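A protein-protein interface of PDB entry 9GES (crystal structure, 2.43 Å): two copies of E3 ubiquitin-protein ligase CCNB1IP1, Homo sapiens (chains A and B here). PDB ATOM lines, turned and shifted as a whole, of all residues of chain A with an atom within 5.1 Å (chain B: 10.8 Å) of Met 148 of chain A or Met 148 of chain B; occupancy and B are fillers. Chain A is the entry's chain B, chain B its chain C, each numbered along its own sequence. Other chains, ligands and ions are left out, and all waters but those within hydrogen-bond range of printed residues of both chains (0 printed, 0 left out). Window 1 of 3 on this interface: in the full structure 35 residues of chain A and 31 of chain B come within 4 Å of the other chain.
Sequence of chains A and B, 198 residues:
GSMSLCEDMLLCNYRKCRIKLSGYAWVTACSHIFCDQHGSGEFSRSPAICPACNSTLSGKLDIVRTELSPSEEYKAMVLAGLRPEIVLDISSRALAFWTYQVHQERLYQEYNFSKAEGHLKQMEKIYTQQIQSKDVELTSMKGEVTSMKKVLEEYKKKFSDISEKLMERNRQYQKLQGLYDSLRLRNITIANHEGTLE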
ATOM      1  N   GLU A 144      -0.660 -11.682  25.241  1.00  0.00           N
ATOM      2  CA  GLU A 144      -1.065 -10.742  26.280  1.00  0.00           C
ATOM      3  C   GLU A 144      -1.973  -9.657  25.714  1.00  0.00           C
ATOM      4  O   GLU A 144      -2.981  -9.300  26.332  1.00  0.00           O
ATOM      5  CB  GLU A 144       0.166 -10.123  26.942  1.00  0.00           C
ATOM      6  CG  GLU A 144       0.995 -11.106  27.754  1.00  0.00           C
ATOM      7  CD  GLU A 144       2.263 -10.484  28.311  1.00  0.00           C
ATOM      8  OE1 GLU A 144       2.570  -9.327  27.951  1.00  0.00           O
ATOM      9  OE2 GLU A 144       2.955 -11.153  29.106  1.00  0.00           O
ATOM     10  N   VAL A 145      -1.638  -9.133  24.531  1.00  0.00           N
ATOM     11  CA  VAL A 145      -2.451  -8.084  23.918  1.00  0.00           C
ATOM     12  C   VAL A 145      -3.860  -8.593  23.643  1.00  0.00           C
ATOM     13  O   VAL A 145      -4.848  -7.878  23.858  1.00  0.00           O
ATOM     14  CB  VAL A 145      -1.772  -7.561  22.638  1.00  0.00           C
ATOM     15  CG1 VAL A 145      -2.734  -6.703  21.830  1.00  0.00           C
ATOM     16  CG2 VAL A 145      -0.525  -6.766  22.989  1.00  0.00           C
ATOM     17  N   THR A 146      -3.979  -9.836  23.169  1.00  0.00           N
ATOM     18  CA  THR A 146      -5.299 -10.414  22.941  1.00  0.00           C
ATOM     19  C   THR A 146      -6.095 -10.496  24.239  1.00  0.00           C
ATOM     20  O   THR A 146      -7.298 -10.211  24.256  1.00  0.00           O
ATOM     21  CB  THR A 146      -5.167 -11.796  22.302  1.00  0.00           C
ATOM     22  OG1 THR A 146      -4.334 -12.630  23.118  1.00  0.00           O
ATOM     23  CG2 THR A 146      -4.556 -11.683  20.910  1.00  0.00           C
ATOM     24  N   SER A 147      -5.438 -10.877  25.337  1.00  0.00           N
ATOM     25  CA  SER A 147      -6.118 -10.920  26.628  1.00  0.00           C
ATOM     26  C   SER A 147      -6.580  -9.532  27.057  1.00  0.00           C
ATOM     27  O   SER A 147      -7.670  -9.382  27.619  1.00  0.00           O
ATOM     28  CB  SER A 147      -5.201 -11.535  27.687  1.00  0.00           C
ATOM     29  OG  SER A 147      -4.024 -10.765  27.850  1.00  0.00           O
ATOM     30  N   MET A 148      -5.763  -8.505  26.804  1.00  0.00           N
ATOM     31  CA  MET A 148      -6.172  -7.141  27.133  1.00  0.00           C
ATOM     32  C   MET A 148      -7.409  -6.735  26.343  1.00  0.00           C
ATOM     33  O   MET A 148      -8.316  -6.089  26.882  1.00  0.00           O
ATOM     34  CB  MET A 148      -5.029  -6.160  26.866  1.00  0.00           C
ATOM     35  CG  MET A 148      -3.696  -6.548  27.492  1.00  0.00           C
ATOM     36  SD  MET A 148      -3.703  -6.686  29.289  1.00  0.00           S
ATOM     37  CE  MET A 148      -3.686  -4.960  29.755  1.00  0.00           C
ATOM     38  N   LYS A 149      -7.460  -7.100  25.059  1.00  0.00           N
ATOM     39  CA  LYS A 149      -8.620  -6.766  24.239  1.00  0.00           C
ATOM     40  C   LYS A 149      -9.871  -7.492  24.723  1.00  0.00           C
ATOM     41  O   LYS A 149     -10.969  -6.924  24.704  1.00  0.00           O
ATOM     42  CB  LYS A 149      -8.336  -7.088  22.773  1.00  0.00           C
ATOM     43  CG  LYS A 149      -7.210  -6.263  22.172  1.00  0.00           C
ATOM     44  CD  LYS A 149      -7.088  -6.483  20.674  1.00  0.00           C
ATOM     45  CE  LYS A 149      -6.017  -5.584  20.076  1.00  0.00           C
ATOM     46  NZ  LYS A 149      -5.911  -5.752  18.601  1.00  0.00           N
ATOM     47  N   LYS A 150      -9.727  -8.750  25.149  1.00  0.00           N
ATOM     48  CA  LYS A 150     -10.866  -9.475  25.705  1.00  0.00           C
ATOM     49  C   LYS A 150     -11.387  -8.794  26.961  1.00  0.00           C
ATOM     50  O   LYS A 150     -12.603  -8.671  27.152  1.00  0.00           O
ATOM     51  CB  LYS A 150     -10.477 -10.922  26.007  1.00  0.00           C
ATOM     52  CG  LYS A 150     -10.011 -11.710  24.800  1.00  0.00           C
ATOM     53  CD  LYS A 150      -9.231 -12.942  25.224  1.00  0.00           C
ATOM     54  CE  LYS A 150      -8.527 -13.586  24.041  1.00  0.00           C
ATOM     55  NZ  LYS A 150      -7.623 -14.690  24.467  1.00  0.00           N
ATOM     56  N   VAL A 151     -10.481  -8.347  27.834  1.00  0.00           N
ATOM     57  CA  VAL A 151     -10.892  -7.631  29.037  1.00  0.00           C
ATOM     58  C   VAL A 151     -11.568  -6.315  28.669  1.00  0.00           C
ATOM     59  O   VAL A 151     -12.541  -5.900  29.310  1.00  0.00           O
ATOM     60  CB  VAL A 151      -9.685  -7.416  29.968  1.00  0.00           C
ATOM     61  CG1 VAL A 151     -10.093  -6.640  31.206  1.00  0.00           C
ATOM     62  CG2 VAL A 151      -9.081  -8.753  30.365  1.00  0.00           C
ATOM     63  N   LEU A 152     -11.068  -5.641  27.630  1.00  0.00           N
ATOM     64  CA  LEU A 152     -11.674  -4.385  27.194  1.00  0.00           C
ATOM     65  C   LEU A 152     -13.118  -4.588  26.752  1.00  0.00           C
ATOM     66  O   LEU A 152     -14.006  -3.811  27.121  1.00  0.00           O
ATOM     67  CB  LEU A 152     -10.849  -3.768  26.064  1.00  0.00           C
ATOM     68  CG  LEU A 152      -9.798  -2.733  26.462  1.00  0.00           C
ATOM     69  CD1 LEU A 152      -8.960  -2.337  25.260  1.00  0.00           C
ATOM     70  CD2 LEU A 152     -10.465  -1.513  27.074  1.00  0.00           C
ATOM     71  N   SER B 140       8.459  -2.384  19.810  1.00  0.00           N
ATOM     72  CA  SER B 140       7.136  -2.052  19.291  1.00  0.00           C
ATOM     73  C   SER B 140       6.044  -2.797  20.050  1.00  0.00           C
ATOM     74  O   SER B 140       5.010  -2.215  20.401  1.00  0.00           O
ATOM     75  CB  SER B 140       7.061  -2.363  17.796  1.00  0.00           C
ATOM     76  OG  SER B 140       5.762  -2.092  17.291  1.00  0.00           O
ATOM     77  N   MET B 141       6.249  -4.093  20.299  1.00  0.00           N
ATOM     78  CA  MET B 141       5.270  -4.864  21.061  1.00  0.00           C
ATOM     79  C   MET B 141       5.181  -4.378  22.504  1.00  0.00           C
ATOM     80  O   MET B 141       4.088  -4.325  23.079  1.00  0.00           O
ATOM     81  CB  MET B 141       5.614  -6.353  21.015  1.00  0.00           C
ATOM     82  CG  MET B 141       5.272  -7.024  19.699  1.00  0.00           C
ATOM     83  SD  MET B 141       3.534  -6.811  19.275  1.00  0.00           S
ATOM     84  CE  MET B 141       2.725  -7.514  20.711  1.00  0.00           C
ATOM     85  N   LYS B 142       6.321  -4.029  23.106  1.00  0.00           N
ATOM     86  CA  LYS B 142       6.312  -3.505  24.469  1.00  0.00           C
ATOM     87  C   LYS B 142       5.517  -2.208  24.554  1.00  0.00           C
ATOM     88  O   LYS B 142       4.762  -1.995  25.510  1.00  0.00           O
ATOM     89  CB  LYS B 142       7.744  -3.291  24.962  1.00  0.00           C
ATOM     90  CG  LYS B 142       8.527  -4.576  25.166  1.00  0.00           C
ATOM     91  CD  LYS B 142      10.020  -4.300  25.289  1.00  0.00           C
ATOM     92  CE  LYS B 142      10.820  -5.593  25.341  1.00  0.00           C
ATOM     93  NZ  LYS B 142      12.288  -5.344  25.363  1.00  0.00           N
ATOM     94  N   GLY B 143       5.682  -1.325  23.567  1.00  0.00           N
ATOM     95  CA  GLY B 143       4.881  -0.112  23.532  1.00  0.00           C
ATOM     96  C   GLY B 143       3.402  -0.394  23.360  1.00  0.00           C
ATOM     97  O   GLY B 143       2.559   0.262  23.977  1.00  0.00           O
ATOM     98  N   GLU B 144       3.064  -1.373  22.514  1.00  0.00           N
ATOM     99  CA  GLU B 144       1.667  -1.755  22.345  1.00  0.00           C
ATOM    100  C   GLU B 144       1.091  -2.331  23.634  1.00  0.00           C
ATOM    101  O   GLU B 144      -0.057  -2.045  23.989  1.00  0.00           O
ATOM    102  CB  GLU B 144       1.530  -2.757  21.199  1.00  0.00           C
ATOM    103  CG  GLU B 144       1.861  -2.183  19.832  1.00  0.00           C
ATOM    104  CD  GLU B 144       1.849  -3.238  18.743  1.00  0.00           C
ATOM    105  OE1 GLU B 144       1.555  -4.408  19.060  1.00  0.00           O
ATOM    106  OE2 GLU B 144       2.131  -2.900  17.573  1.00  0.00           O
ATOM    107  N   VAL B 145       1.873  -3.148  24.344  1.00  0.00           N
ATOM    108  CA  VAL B 145       1.405  -3.711  25.609  1.00  0.00           C
ATOM    109  C   VAL B 145       1.154  -2.605  26.625  1.00  0.00           C
ATOM    110  O   VAL B 145       0.148  -2.620  27.345  1.00  0.00           O
ATOM    111  CB  VAL B 145       2.407  -4.756  26.137  1.00  0.00           C
ATOM    112  CG1 VAL B 145       2.078  -5.134  27.573  1.00  0.00           C
ATOM    113  CG2 VAL B 145       2.395  -5.993  25.254  1.00  0.00           C
ATOM    114  N   THR B 146       2.060  -1.625  26.699  1.00  0.00           N
ATOM    115  CA  THR B 146       1.856  -0.503  27.609  1.00  0.00           C
ATOM    116  C   THR B 146       0.602   0.281  27.246  1.00  0.00           C
ATOM    117  O   THR B 146      -0.154   0.699  28.130  1.00  0.00           O
ATOM    118  CB  THR B 146       3.078   0.417  27.608  1.00  0.00           C
ATOM    119  OG1 THR B 146       3.368   0.835  26.268  1.00  0.00           O
ATOM    120  CG2 THR B 146       4.288  -0.297  28.195  1.00  0.00           C
ATOM    121  N   SER B 147       0.365   0.491  25.948  1.00  0.00           N
ATOM    122  CA  SER B 147      -0.833   1.209  25.520  1.00  0.00           C
ATOM    123  C   SER B 147      -2.099   0.464  25.923  1.00  0.00           C
ATOM    124  O   SER B 147      -3.073   1.080  26.372  1.00  0.00           O
ATOM    125  CB  SER B 147      -0.800   1.433  24.007  1.00  0.00           C
ATOM    126  OG  SER B 147      -0.846   0.201  23.309  1.00  0.00           O
ATOM    127  N   MET B 148      -2.107  -0.862  25.763  1.00  0.00           N
ATOM    128  CA  MET B 148      -3.272  -1.646  26.165  1.00  0.00           C
ATOM    129  C   MET B 148      -3.495  -1.572  27.671  1.00  0.00           C
ATOM    130  O   MET B 148      -4.640  -1.483  28.132  1.00  0.00           O
ATOM    131  CB  MET B 148      -3.113  -3.098  25.713  1.00  0.00           C
ATOM    132  CG  MET B 148      -2.984  -3.274  24.208  1.00  0.00           C
ATOM    133  SD  MET B 148      -4.353  -2.531  23.299  1.00  0.00           S
ATOM    134  CE  MET B 148      -5.742  -3.434  23.976  1.00  0.00           C
ATOM    135  N   LYS B 149      -2.414  -1.613  28.455  1.00  0.00           N
ATOM    136  CA  LYS B 149      -2.546  -1.490  29.904  1.00  0.00           C
ATOM    137  C   LYS B 149      -3.112  -0.130  30.294  1.00  0.00           C
ATOM    138  O   LYS B 149      -3.973  -0.038  31.177  1.00  0.00           O
ATOM    139  CB  LYS B 149      -1.193  -1.720  30.578  1.00  0.00           C
ATOM    140  CG  LYS B 149      -0.659  -3.135  30.445  1.00  0.00           C
ATOM    141  CD  LYS B 149       0.615  -3.323  31.251  1.00  0.00           C
ATOM    142  CE  LYS B 149       1.103  -4.760  31.177  1.00  0.00           C
ATOM    143  NZ  LYS B 149       2.328  -4.976  31.993  1.00  0.00           N
ATOM    144  N   LYS B 150      -2.636   0.939  29.650  1.00  0.00           N
ATOM    145  CA  LYS B 150      -3.147   2.274  29.949  1.00  0.00           C
ATOM    146  C   LYS B 150      -4.624   2.392  29.594  1.00  0.00           C
ATOM    147  O   LYS B 150      -5.412   2.950  30.367  1.00  0.00           O
ATOM    148  CB  LYS B 150      -2.328   3.327  29.203  1.00  0.00           C
ATOM    149  CG  LYS B 150      -0.862   3.379  29.607  1.00  0.00           C
ATOM    150  CD  LYS B 150      -0.012   4.000  28.507  1.00  0.00           C
ATOM    151  CE  LYS B 150       1.471   3.798  28.774  1.00  0.00           C
ATOM    152  NZ  LYS B 150       2.315   4.239  27.628  1.00  0.00           N
ATOM    153  N   VAL B 151      -5.021   1.863  28.434  1.00  0.00           N
ATOM    154  CA  VAL B 151      -6.418   1.944  28.013  1.00  0.00           C
ATOM    155  C   VAL B 151      -7.318   1.189  28.983  1.00  0.00           C
ATOM    156  O   VAL B 151      -8.390   1.676  29.365  1.00  0.00           O
ATOM    157  CB  VAL B 151      -6.573   1.418  26.574  1.00  0.00           C
ATOM    158  CG1 VAL B 151      -8.046   1.265  26.220  1.00  0.00           C
ATOM    159  CG2 VAL B 151      -5.886   2.352  25.593  1.00  0.00           C
ATOM    160  N   LEU B 152      -6.900  -0.010  29.396  1.00  0.00           N
ATOM    161  CA  LEU B 152      -7.719  -0.804  30.308  1.00  0.00           C
ATOM    162  C   LEU B 152      -7.882  -0.114  31.657  1.00  0.00           C
ATOM    163  O   LEU B 152      -8.973  -0.124  32.237  1.00  0.00           O
ATOM    164  CB  LEU B 152      -7.117  -2.198  30.479  1.00  0.00           C
ATOM    165  CG  LEU B 152      -7.863  -3.282  29.702  1.00  0.00           C
ATOM    166  CD1 LEU B 152      -7.249  -4.649  29.939  1.00  0.00           C
ATOM    167  CD2 LEU B 152      -9.332  -3.272  30.092  1.00  0.00           C
ATOM    168  N   GLU B 153      -6.808   0.487  32.176  1.00  0.00           N
ATOM    169  CA  GLU B 153      -6.916   1.227  33.430  1.00  0.00           C
ATOM    170  C   GLU B 153      -7.832   2.436  33.281  1.00  0.00           C
ATOM    171  O   GLU B 153      -8.566   2.785  34.213  1.00  0.00           O
ATOM    172  CB  GLU B 153      -5.533   1.657  33.921  1.00  0.00           C
ATOM    173  CG  GLU B 153      -4.753   0.548  34.613  1.00  0.00           C
ATOM    174  CD  GLU B 153      -3.590   1.073  35.434  1.00  0.00           C
ATOM    175  OE1 GLU B 153      -3.362   2.303  35.429  1.00  0.00           O
ATOM    176  OE2 GLU B 153      -2.905   0.258  36.087  1.00  0.00           O
ATOM    177  N   GLU B 154      -7.796   3.095  32.119  1.00  0.00           N
ATOM    178  CA  GLU B 154      -8.711   4.205  31.869  1.00  0.00           C
ATOM    179  C   GLU B 154     -10.161   3.739  31.912  1.00  0.00           C
ATOM    180  O   GLU B 154     -11.016   4.389  32.525  1.00  0.00           O
ATOM    181  CB  GLU B 154      -8.398   4.852  30.519  1.00  0.00           C
ATOM    182  CG  GLU B 154      -7.070   5.584  30.464  1.00  0.00           C
ATOM    183  CD  GLU B 154      -6.675   5.951  29.046  1.00  0.00           C
ATOM    184  OE1 GLU B 154      -7.535   5.854  28.145  1.00  0.00           O
ATOM    185  OE2 GLU B 154      -5.504   6.329  28.830  1.00  0.00           O
ATOM    186  N   TYR B 155     -10.456   2.610  31.262  1.00  0.00           N
ATOM    187  CA  TYR B 155     -11.821   2.091  31.261  1.00  0.00           C
ATOM    188  C   TYR B 155     -12.243   1.625  32.648  1.00  0.00           C
ATOM    189  O   TYR B 155     -13.403   1.798  33.040  1.00  0.00           O
ATOM    190  CB  TYR B 155     -11.951   0.955  30.246  1.00  0.00           C
ATOM    191  CG  TYR B 155     -12.217   1.423  28.833  1.00  0.00           C
ATOM    192  CD1 TYR B 155     -11.231   2.063  28.094  1.00  0.00           C
ATOM    193  CD2 TYR B 155     -13.455   1.218  28.235  1.00  0.00           C
ATOM    194  CE1 TYR B 155     -11.469   2.491  26.801  1.00  0.00           C
ATOM    195  CE2 TYR B 155     -13.703   1.641  26.941  1.00  0.00           C
ATOM    196  CZ  TYR B 155     -12.707   2.277  26.229  1.00  0.00           C
ATOM    197  OH  TYR B 155     -12.949   2.700  24.942  1.00  0.00           O
ATOM    198  N   LYS B 156     -11.319   1.026  33.405  1.00  0.00           N
ATOM    199  CA  LYS B 156     -11.645   0.612  34.766  1.00  0.00           C
ATOM    200  C   LYS B 156     -11.990   1.814  35.636  1.00  0.00           C
ATOM    201  O   LYS B 156     -12.936   1.763  36.431  1.00  0.00           O
ATOM    202  CB  LYS B 156     -10.483  -0.177  35.372  1.00  0.00           C
ATOM    203  CG  LYS B 156     -10.256  -1.535  34.724  1.00  0.00           C
ATOM    204  CD  LYS B 156      -9.142  -2.306  35.411  1.00  0.00           C
ATOM    205  CE  LYS B 156      -8.941  -3.665  34.765  1.00  0.00           C
ATOM    206  NZ  LYS B 156      -7.879  -4.452  35.448  1.00  0.00           N
ATOM    207  N   LYS B 157     -11.233   2.906  35.499  1.00  0.00           N
ATOM    208  CA  LYS B 157     -11.550   4.121  36.244  1.00  0.00           C
ATOM    209  C   LYS B 157     -12.892   4.700  35.811  1.00  0.00           C
ATOM    210  O   LYS B 157     -13.661   5.192  36.645  1.00  0.00           O
ATOM    211  CB  LYS B 157     -10.431   5.148  36.071  1.00  0.00           C
ATOM    212  CG  LYS B 157      -9.100   4.708  36.662  1.00  0.00           C
ATOM    213  CD  LYS B 157      -7.952   5.556  36.140  1.00  0.00           C
ATOM    214  CE  LYS B 157      -6.606   4.981  36.554  1.00  0.00           C
ATOM    215  NZ  LYS B 157      -5.469   5.741  35.966  1.00  0.00           N
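Among the printed residues, pairs that only touch across the chains: Val 145 of chain A with Val 145 of chain B (3.8 Å), Met 148 of chain A with Met 148 of chain B (3.8 Å), Met 148 of chain A with Lys 149 of chain B (3.6 Å), Met 148 of chain A with Leu 152 of chain B (3.5 Å), Lys 149 of chain A with Met 148 of chain B (3.7 Å), Val 151 of chain A with Leu 152 of chain B (3.6 Å), Leu 152 of chain A with Met 148 of chain B (3.6 Å), Leu 152 of chain A with Val 151 of chain B (3.8 Å), Leu 152 of chain A with Leu 152 of chain B (3.7 Å) and Leu 152 of chain A with Tyr 155 of chain B (3.8 Å).
No residue of chain B comes within 4 Å of Ser 147 of chain A. Met 148 of chain A touches three residues of chain B. Of chain B, only Met 148 comes within 4 Å of Lys 149 of chain A. Val 151 of chain A touches one residue of chain B. Leu 152 of chain A touches just these residues of chain B: Met 148 (3.6 Å), Val 151 (3.8 Å), Leu 152 (3.7 Å) and Tyr 155 (3.8 Å). Met 141 of chain B touches none of the printed residues of chain A. Printed residues of chain A within 4 Å of Val 145 of chain B: Val 145 (3.8 Å). Of chain A, only Met 148, Lys 149 and Leu 152 come within 4 Å of Met 148 of chain B. Of the printed residues of chain A, Lys 149 of chain B touches Met 148. Printed residues of chain A within 4 Å of Val 151 of chain B: Leu 152 (3.8 Å). The nearest residue of chain A that does not touch Met 148 of chain B is Val 145 of chain A (4.2 Å). The nearest printed residue of chain A that does not touch Tyr 155 of chain B is Val 151 of chain A (6.9 Å).
Printed residues of chain A that touch a printed residue of chain B: Val 145, Met 148, Lys 149, Val 151 and Leu 152. Along chain A the printed residues that touch a printed residue of chain B span positions 145 to 152. Among the printed residues, 10 pairs touch across the chains. Among the printed residues, no Asp or Glu carboxylate lies within 4 Å of a Lys or Arg side-chain nitrogen of the other chain.
Val 145 of chain B touches its own counterpart, Val 145 of chain A. Met 148 of chain B touches its own counterpart, Met 148 of chain A. Met 148 of chain A touches Lys 149 of chain B, and with the chains exchanged Lys 149 of chain A touches Met 148 of chain B. Leu 152 of chain A touches its own counterpart, Leu 152 of chain B. Of the 10 pairs that touch across the chains among the printed residues, 9 have their exchanged pair printed and touching as well.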
